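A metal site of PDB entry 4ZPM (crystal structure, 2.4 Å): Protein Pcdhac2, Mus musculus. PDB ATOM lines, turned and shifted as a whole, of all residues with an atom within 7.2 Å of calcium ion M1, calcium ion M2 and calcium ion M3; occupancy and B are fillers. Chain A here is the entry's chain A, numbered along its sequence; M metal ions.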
ATOM      1  N   GLU A   8      30.808  20.419   0.123  1.00  0.00           N
ATOM      2  CA  GLU A   8      31.659  21.136   1.064  1.00  0.00           C
ATOM      3  C   GLU A   8      33.104  20.609   1.038  1.00  0.00           C
ATOM      4  O   GLU A   8      33.360  19.516   0.525  1.00  0.00           O
ATOM      5  CB  GLU A   8      31.090  21.034   2.477  1.00  0.00           C
ATOM      6  CG  GLU A   8      31.156  19.628   3.044  1.00  0.00           C
ATOM      7  CD  GLU A   8      30.660  19.534   4.476  1.00  0.00           C
ATOM      8  OE1 GLU A   8      31.129  20.326   5.327  1.00  0.00           O
ATOM      9  OE2 GLU A   8      29.805  18.663   4.752  1.00  0.00           O
ATOM     10  N   GLU A   9      34.014  21.407   1.567  1.00  0.00           N
ATOM     11  CA  GLU A   9      35.395  20.990   1.849  1.00  0.00           C
ATOM     12  C   GLU A   9      36.234  20.654   0.614  1.00  0.00           C
ATOM     13  O   GLU A   9      37.264  19.989   0.739  1.00  0.00           O
ATOM     14  CB  GLU A   9      35.380  19.767   2.790  1.00  0.00           C
ATOM     15  CG  GLU A   9      34.649  19.988   4.110  1.00  0.00           C
ATOM     16  CD  GLU A   9      35.395  20.907   5.067  1.00  0.00           C
ATOM     17  OE1 GLU A   9      36.545  21.285   4.756  1.00  0.00           O
ATOM     18  OE2 GLU A   9      34.814  21.252   6.118  1.00  0.00           O
ATOM     19  N   ARG A  62      38.071  27.269   1.744  1.00  0.00           N
ATOM     20  CA  ARG A  62      37.468  26.099   2.369  1.00  0.00           C
ATOM     21  C   ARG A  62      36.046  26.408   2.806  1.00  0.00           C
ATOM     22  O   ARG A  62      35.798  27.360   3.558  1.00  0.00           O
ATOM     23  CB  ARG A  62      38.300  25.630   3.568  1.00  0.00           C
ATOM     24  CG  ARG A  62      37.564  24.635   4.470  1.00  0.00           C
ATOM     25  CD  ARG A  62      38.318  24.419   5.774  1.00  0.00           C
ATOM     26  NE  ARG A  62      37.791  23.286   6.526  1.00  0.00           N
ATOM     27  CZ  ARG A  62      37.124  23.400   7.674  1.00  0.00           C
ATOM     28  NH1 ARG A  62      36.905  24.596   8.202  1.00  0.00           N
ATOM     29  NH2 ARG A  62      36.670  22.311   8.288  1.00  0.00           N
ATOM     30  N   ILE A  63      35.100  25.602   2.340  1.00  0.00           N
ATOM     31  CA  ILE A  63      33.695  25.758   2.681  1.00  0.00           C
ATOM     32  C   ILE A  63      33.253  24.639   3.610  1.00  0.00           C
ATOM     33  O   ILE A  63      33.079  23.505   3.167  1.00  0.00           O
ATOM     34  CB  ILE A  63      32.814  25.776   1.423  1.00  0.00           C
ATOM     35  CG1 ILE A  63      33.330  26.805   0.407  1.00  0.00           C
ATOM     36  CG2 ILE A  63      31.356  26.044   1.785  1.00  0.00           C
ATOM     37  CD1 ILE A  63      32.417  26.999  -0.782  1.00  0.00           C
ATOM     38  N   ASP A  64      33.079  24.940   4.892  1.00  0.00           N
ATOM     39  CA  ASP A  64      32.640  23.944   5.887  1.00  0.00           C
ATOM     40  C   ASP A  64      31.159  24.101   6.201  1.00  0.00           C
ATOM     41  O   ASP A  64      30.761  25.043   6.894  1.00  0.00           O
ATOM     42  CB  ASP A  64      33.468  24.067   7.168  1.00  0.00           C
ATOM     43  CG  ASP A  64      32.979  23.151   8.290  1.00  0.00           C
ATOM     44  OD1 ASP A  64      32.454  22.063   7.994  1.00  0.00           O
ATOM     45  OD2 ASP A  64      33.135  23.527   9.475  1.00  0.00           O
ATOM     46  N   ARG A  65      30.350  23.178   5.692  1.00  0.00           N
ATOM     47  CA  ARG A  65      28.897  23.246   5.872  1.00  0.00           C
ATOM     48  C   ARG A  65      28.492  23.197   7.339  1.00  0.00           C
ATOM     49  O   ARG A  65      27.517  23.840   7.738  1.00  0.00           O
ATOM     50  CB  ARG A  65      28.218  22.105   5.114  1.00  0.00           C
ATOM     51  CG  ARG A  65      26.703  22.274   5.007  1.00  0.00           C
ATOM     52  CD  ARG A  65      25.984  20.937   5.083  1.00  0.00           C
ATOM     53  NE  ARG A  65      26.258  20.243   6.338  1.00  0.00           N
ATOM     54  CZ  ARG A  65      25.663  20.524   7.492  1.00  0.00           C
ATOM     55  NH1 ARG A  65      24.754  21.494   7.548  1.00  0.00           N
ATOM     56  NH2 ARG A  65      25.974  19.848   8.595  1.00  0.00           N
ATOM     57  N   GLU A  66      29.240  22.456   8.146  1.00  0.00           N
ATOM     58  CA  GLU A  66      28.950  22.341   9.567  1.00  0.00           C
ATOM     59  C   GLU A  66      29.054  23.686  10.272  1.00  0.00           C
ATOM     60  O   GLU A  66      28.210  24.037  11.095  1.00  0.00           O
ATOM     61  CB  GLU A  66      29.866  21.317  10.239  1.00  0.00           C
ATOM     62  CG  GLU A  66      29.403  19.861  10.101  1.00  0.00           C
ATOM     63  CD  GLU A  66      29.554  19.315   8.700  1.00  0.00           C
ATOM     64  OE1 GLU A  66      28.531  19.016   8.045  1.00  0.00           O
ATOM     65  OE2 GLU A  66      30.705  19.156   8.241  1.00  0.00           O
ATOM     66  N   ALA A  67      30.097  24.452   9.954  1.00  0.00           N
ATOM     67  CA  ALA A  67      30.276  25.773  10.539  1.00  0.00           C
ATOM     68  C   ALA A  67      29.232  26.758  10.023  1.00  0.00           C
ATOM     69  O   ALA A  67      28.735  27.594  10.776  1.00  0.00           O
ATOM     70  CB  ALA A  67      31.673  26.290  10.266  1.00  0.00           C
ATOM     71  N   LEU A  97      26.460  21.070  -0.530  1.00  0.00           N
ATOM     72  CA  LEU A  97      26.106  19.688  -0.227  1.00  0.00           C
ATOM     73  C   LEU A  97      26.910  19.186   0.962  1.00  0.00           C
ATOM     74  O   LEU A  97      28.059  19.564   1.147  1.00  0.00           O
ATOM     75  CB  LEU A  97      26.351  18.784  -1.440  1.00  0.00           C
ATOM     76  CG  LEU A  97      25.705  19.200  -2.761  1.00  0.00           C
ATOM     77  CD1 LEU A  97      26.057  18.214  -3.860  1.00  0.00           C
ATOM     78  CD2 LEU A  97      24.201  19.325  -2.601  1.00  0.00           C
ATOM     79  N   ASP A  98      26.274  18.352   1.780  1.00  0.00           N
ATOM     80  CA  ASP A  98      26.957  17.785   2.927  1.00  0.00           C
ATOM     81  C   ASP A  98      27.703  16.510   2.566  1.00  0.00           C
ATOM     82  O   ASP A  98      27.179  15.675   1.840  1.00  0.00           O
ATOM     83  CB  ASP A  98      25.963  17.504   4.060  1.00  0.00           C
ATOM     84  CG  ASP A  98      26.598  16.788   5.229  1.00  0.00           C
ATOM     85  OD1 ASP A  98      27.415  17.426   5.929  1.00  0.00           O
ATOM     86  OD2 ASP A  98      26.271  15.609   5.457  1.00  0.00           O
ATOM     87  N   ILE A  99      28.923  16.387   3.060  1.00  0.00           N
ATOM     88  CA  ILE A  99      29.667  15.137   2.939  1.00  0.00           C
ATOM     89  C   ILE A  99      29.823  14.510   4.317  1.00  0.00           C
ATOM     90  O   ILE A  99      29.655  15.184   5.344  1.00  0.00           O
ATOM     91  CB  ILE A  99      31.052  15.345   2.292  1.00  0.00           C
ATOM     92  CG1 ILE A  99      31.973  16.133   3.226  1.00  0.00           C
ATOM     93  CG2 ILE A  99      30.911  16.040   0.946  1.00  0.00           C
ATOM     94  CD1 ILE A  99      33.369  16.357   2.663  1.00  0.00           C
ATOM     95  N   ASN A 100      30.133  13.220   4.344  1.00  0.00           N
ATOM     96  CA  ASN A 100      30.283  12.498   5.601  1.00  0.00           C
ATOM     97  C   ASN A 100      31.671  12.636   6.194  1.00  0.00           C
ATOM     98  O   ASN A 100      32.416  11.661   6.286  1.00  0.00           O
ATOM     99  CB  ASN A 100      29.951  11.017   5.398  1.00  0.00           C
ATOM    100  CG  ASN A 100      29.568  10.330   6.691  1.00  0.00           C
ATOM    101  OD1 ASN A 100      28.968  10.952   7.566  1.00  0.00           O
ATOM    102  ND2 ASN A 100      29.913   9.055   6.818  1.00  0.00           N
ATOM    103  N   ASP A 101      32.030  13.855   6.601  1.00  0.00           N
ATOM    104  CA  ASP A 101      33.367  14.112   7.113  1.00  0.00           C
ATOM    105  C   ASP A 101      33.388  14.219   8.635  1.00  0.00           C
ATOM    106  O   ASP A 101      34.345  14.712   9.225  1.00  0.00           O
ATOM    107  CB  ASP A 101      33.948  15.390   6.477  1.00  0.00           C
ATOM    108  CG  ASP A 101      33.050  16.599   6.681  1.00  0.00           C
ATOM    109  OD1 ASP A 101      31.830  16.416   6.883  1.00  0.00           O
ATOM    110  OD2 ASP A 101      33.567  17.738   6.609  1.00  0.00           O
ATOM    111  N   ASN A 102      32.320  13.754   9.268  1.00  0.00           N
ATOM    112  CA  ASN A 102      32.258  13.698  10.724  1.00  0.00           C
ATOM    113  C   ASN A 102      31.750  12.344  11.212  1.00  0.00           C
ATOM    114  O   ASN A 102      30.896  11.728  10.578  1.00  0.00           O
ATOM    115  CB  ASN A 102      31.376  14.817  11.281  1.00  0.00           C
ATOM    116  CG  ASN A 102      31.970  16.192  11.054  1.00  0.00           C
ATOM    117  OD1 ASN A 102      32.740  16.690  11.874  1.00  0.00           O
ATOM    118  ND2 ASN A 102      31.613  16.801   9.936  1.00  0.00           N
ATOM    119  N   SER A 103      32.288  11.886  12.339  1.00  0.00           N
ATOM    120  CA  SER A 103      31.864  10.629  12.925  1.00  0.00           C
ATOM    121  C   SER A 103      30.915  10.849  14.100  1.00  0.00           C
ATOM    122  O   SER A 103      30.995  11.879  14.770  1.00  0.00           O
ATOM    123  CB  SER A 103      33.087   9.820  13.383  1.00  0.00           C
ATOM    124  OG  SER A 103      33.761   9.252  12.282  1.00  0.00           O
ATOM    125  N   PRO A 104      30.006   9.897  14.337  1.00  0.00           N
ATOM    126  CA  PRO A 104      29.144   9.916  15.522  1.00  0.00           C
ATOM    127  C   PRO A 104      29.950   9.945  16.818  1.00  0.00           C
ATOM    128  O   PRO A 104      30.929   9.210  16.936  1.00  0.00           O
ATOM    129  CB  PRO A 104      28.349   8.613  15.400  1.00  0.00           C
ATOM    130  CG  PRO A 104      28.288   8.375  13.941  1.00  0.00           C
ATOM    131  CD  PRO A 104      29.643   8.792  13.437  1.00  0.00           C
ATOM    132  N   ASP A 132      25.996  13.494  15.779  1.00  0.00           N
ATOM    133  CA  ASP A 132      26.760  13.592  14.531  1.00  0.00           C
ATOM    134  C   ASP A 132      26.451  14.916  13.839  1.00  0.00           C
ATOM    135  O   ASP A 132      25.346  15.138  13.372  1.00  0.00           O
ATOM    136  CB  ASP A 132      26.436  12.417  13.596  1.00  0.00           C
ATOM    137  CG  ASP A 132      27.425  12.289  12.444  1.00  0.00           C
ATOM    138  OD1 ASP A 132      27.842  13.317  11.866  1.00  0.00           O
ATOM    139  OD2 ASP A 132      27.790  11.146  12.105  1.00  0.00           O
ATOM    140  N   PRO A 133      27.458  15.812  13.791  1.00  0.00           N
ATOM    141  CA  PRO A 133      27.249  17.161  13.252  1.00  0.00           C
ATOM    142  C   PRO A 133      26.876  17.190  11.763  1.00  0.00           C
ATOM    143  O   PRO A 133      26.494  18.248  11.267  1.00  0.00           O
ATOM    144  CB  PRO A 133      28.605  17.847  13.494  1.00  0.00           C
ATOM    145  CG  PRO A 133      29.587  16.738  13.646  1.00  0.00           C
ATOM    146  CD  PRO A 133      28.832  15.597  14.269  1.00  0.00           C
ATOM    147  N   ASP A 134      26.969  16.059  11.072  1.00  0.00           N
ATOM    148  CA  ASP A 134      26.518  15.986   9.687  1.00  0.00           C
ATOM    149  C   ASP A 134      24.989  15.979   9.651  1.00  0.00           C
ATOM    150  O   ASP A 134      24.339  15.997  10.694  1.00  0.00           O
ATOM    151  CB  ASP A 134      27.063  14.753   8.974  1.00  0.00           C
ATOM    152  CG  ASP A 134      28.567  14.776   8.825  1.00  0.00           C
ATOM    153  OD1 ASP A 134      29.182  15.840   9.053  1.00  0.00           O
ATOM    154  OD2 ASP A 134      29.144  13.726   8.486  1.00  0.00           O
ATOM    155  N   VAL A 135      24.423  15.946   8.446  1.00  0.00           N
ATOM    156  CA  VAL A 135      22.976  16.023   8.273  1.00  0.00           C
ATOM    157  C   VAL A 135      22.481  14.933   7.340  1.00  0.00           C
ATOM    158  O   VAL A 135      23.261  14.328   6.604  1.00  0.00           O
ATOM    159  CB  VAL A 135      22.537  17.406   7.719  1.00  0.00           C
ATOM    160  CG1 VAL A 135      22.786  18.496   8.757  1.00  0.00           C
ATOM    161  CG2 VAL A 135      23.257  17.709   6.413  1.00  0.00           C
ATOM    162  N   ALA A 137      21.403  11.535   5.718  1.00  0.00           N
ATOM    163  CA  ALA A 137      21.925  10.177   5.821  1.00  0.00           C
ATOM    164  C   ALA A 137      23.286  10.133   6.514  1.00  0.00           C
ATOM    165  O   ALA A 137      23.644   9.140   7.134  1.00  0.00           O
ATOM    166  CB  ALA A 137      22.021   9.548   4.444  1.00  0.00           C
ATOM    167  N   ASN A 138      24.040  11.216   6.396  1.00  0.00           N
ATOM    168  CA  ASN A 138      25.377  11.284   6.983  1.00  0.00           C
ATOM    169  C   ASN A 138      25.366  11.374   8.512  1.00  0.00           C
ATOM    170  O   ASN A 138      26.417  11.269   9.150  1.00  0.00           O
ATOM    171  CB  ASN A 138      26.146  12.466   6.405  1.00  0.00           C
ATOM    172  CG  ASN A 138      26.493  12.276   4.945  1.00  0.00           C
ATOM    173  OD1 ASN A 138      26.611  11.161   4.454  1.00  0.00           O
ATOM    174  ND2 ASN A 138      26.657  13.387   4.227  1.00  0.00           N
ATOM    175  N   SER A 139      24.195  11.573   9.100  1.00  0.00           N
ATOM    176  CA  SER A 139      24.069  11.638  10.546  1.00  0.00           C
ATOM    177  C   SER A 139      23.792  10.258  11.134  1.00  0.00           C
ATOM    178  O   SER A 139      23.668   9.283  10.395  1.00  0.00           O
ATOM    179  CB  SER A 139      22.959  12.627  10.951  1.00  0.00           C
ATOM    180  OG  SER A 139      23.101  13.014  12.305  1.00  0.00           O
ATOM    181  N   VAL A 140      23.674  10.185  12.460  1.00  0.00           N
ATOM    182  CA  VAL A 140      23.452   8.900  13.137  1.00  0.00           C
ATOM    183  C   VAL A 140      22.156   8.216  12.698  1.00  0.00           C
ATOM    184  O   VAL A 140      21.085   8.818  12.738  1.00  0.00           O
ATOM    185  CB  VAL A 140      23.430   9.077  14.651  1.00  0.00           C
ATOM    186  CG1 VAL A 140      23.151   7.749  15.346  1.00  0.00           C
ATOM    187  CG2 VAL A 140      24.747   9.674  15.128  1.00  0.00           C
ATOM    188  N   ASP A 189      26.576   5.987  11.267  1.00  0.00           N
ATOM    189  CA  ASP A 189      25.848   6.854  10.340  1.00  0.00           C
ATOM    190  C   ASP A 189      25.529   6.103   9.055  1.00  0.00           C
ATOM    191  O   ASP A 189      25.931   4.951   8.885  1.00  0.00           O
ATOM    192  CB  ASP A 189      26.611   8.158  10.050  1.00  0.00           C
ATOM    193  CG  ASP A 189      27.980   7.947   9.399  1.00  0.00           C
ATOM    194  OD1 ASP A 189      28.165   7.003   8.591  1.00  0.00           O
ATOM    195  OD2 ASP A 189      28.885   8.757   9.689  1.00  0.00           O
ATOM    196  N   GLY A 190      24.815   6.752   8.143  1.00  0.00           N
ATOM    197  CA  GLY A 190      24.387   6.119   6.909  1.00  0.00           C
ATOM    198  C   GLY A 190      25.221   6.479   5.702  1.00  0.00           C
ATOM    199  O   GLY A 190      24.855   6.171   4.563  1.00  0.00           O
ATOM    200  N   GLY A 191      26.347   7.140   5.939  1.00  0.00           N
ATOM    201  CA  GLY A 191      27.285   7.453   4.876  1.00  0.00           C
ATOM    202  C   GLY A 191      27.963   6.199   4.355  1.00  0.00           C
ATOM    203  O   GLY A 191      27.976   5.179   5.034  1.00  0.00           O
ATOM    204  N   ARG A 195      30.645   5.633   9.151  1.00  0.00           N
ATOM    205  CA  ARG A 195      31.557   6.057  10.209  1.00  0.00           C
ATOM    206  C   ARG A 195      30.928   5.761  11.571  1.00  0.00           C
ATOM    207  O   ARG A 195      29.708   5.851  11.742  1.00  0.00           O
ATOM    208  CB  ARG A 195      31.897   7.537  10.068  1.00  0.00           C
ATOM    209  CG  ARG A 195      32.571   7.861   8.741  1.00  0.00           C
ATOM    210  CD  ARG A 195      32.898   9.344   8.606  1.00  0.00           C
ATOM    211  NE  ARG A 195      33.791   9.806   9.656  1.00  0.00           N
ATOM    212  CZ  ARG A 195      34.716  10.750   9.495  1.00  0.00           C
ATOM    213  NH1 ARG A 195      34.863  11.331   8.310  1.00  0.00           N
ATOM    214  NH2 ARG A 195      35.490  11.106  10.511  1.00  0.00           N
HETATM  215 CA    CA M   1      32.740  19.922   7.232  1.00  0.00          CA
HETATM  216 CA    CA M   2      29.628  17.213   6.825  1.00  0.00          CA
HETATM  217 CA    CA M   3      28.727  11.520   9.826  1.00  0.00          CA
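OD2 of Asp 64 lies within salt-bridge range of NH2 of Arg 62.
The backbone NH (N) of Ala 67 is in hydrogen-bond range of the side-chain carboxylate (OD2) of Asp 64 (3.2 Å).
ND2 of Asn 102 sits close to OD1 of Asp 101 (3.1 Å).
The side-chain amide nitrogen (ND2) of Asn 102 sits close to the side-chain carboxylate (OE2) of Glu 66.
NH2 of Arg 65 sits close to OE1 of Glu 66.
The backbone NH (N) of Glu 8 lies within hydrogen-bond range of the backbone carbonyl oxygen (O) of Leu 97.
The backbone carbonyl oxygen (O) of Ile 63 lies within hydrogen-bond range of the backbone NH (N) of Glu 9 (2.8 Å).
The side-chain carboxylate (OD1) of Asp 189 is in hydrogen-bond range of the backbone NH (N) of Arg 195 (2.9 Å).
Within 4 Å of calcium ion M1: Glu 8, Glu 9, Asp 64, Glu 66 and Asp 101.
The nearest printed residue that does not touch calcium ion M1 is Asn 102 (4.3 Å).
Within 4 Å of calcium ion M2: Glu 8, Glu 66, Asp 98, Ile 99, Asp 101, Asn 102 and Asp 134.
Of the 28 residues printed, 6 come within 4 Å of calcium ion M3.
Along chain A the residues within 4 Å of calcium ion M3 span positions 100 to 189.
The side-chain carboxylate (OD1) of Asp 64 binds calcium ion M1, at 2.3 Å.
Calcium ion M1 is bound by OE2 of Glu 66.
Calcium ion M1 is bound by the side-chain carboxylate (OD2) of Asp 101.
Calcium ion M1 is bound by OE1 of Glu 8 (2.5 Å).
The side-chain carboxylate (OE2) of Glu 9 is bound to calcium ion M1.
Calcium ion M2 is bound by OD1 of Asp 101 (2.3 Å), OD1 of Asp 98 (2.4 Å), OE1 of Glu 66 (2.4 Å), O of Ile 99 (2.5 Å), OE2 of Glu 8 (2.5 Å), OE2 of Glu 66 (2.6 Å) and OD1 of Asp 134 (2.7 Å).
The backbone carbonyl oxygen (O) of Asn 102 is bound to calcium ion M3 (2.3 Å).
OD1 of Asn 100 binds calcium ion M3, 2.3 Å away.
The backbone carbonyl oxygen (O) of Asn 138 binds calcium ion M3 (2.4 Å).
OD2 of Asp 132 is bound to calcium ion M3 (2.5 Å).
OD2 of Asp 134 binds calcium ion M3 (2.6 Å).
OD2 of Asp 189 is bound to calcium ion M3 (2.8 Å).
Calcium ion M3 is bound by the side-chain carboxylate (OD1) of Asp 132.
Calcium ion M3 has seven donor atoms within binding distance.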
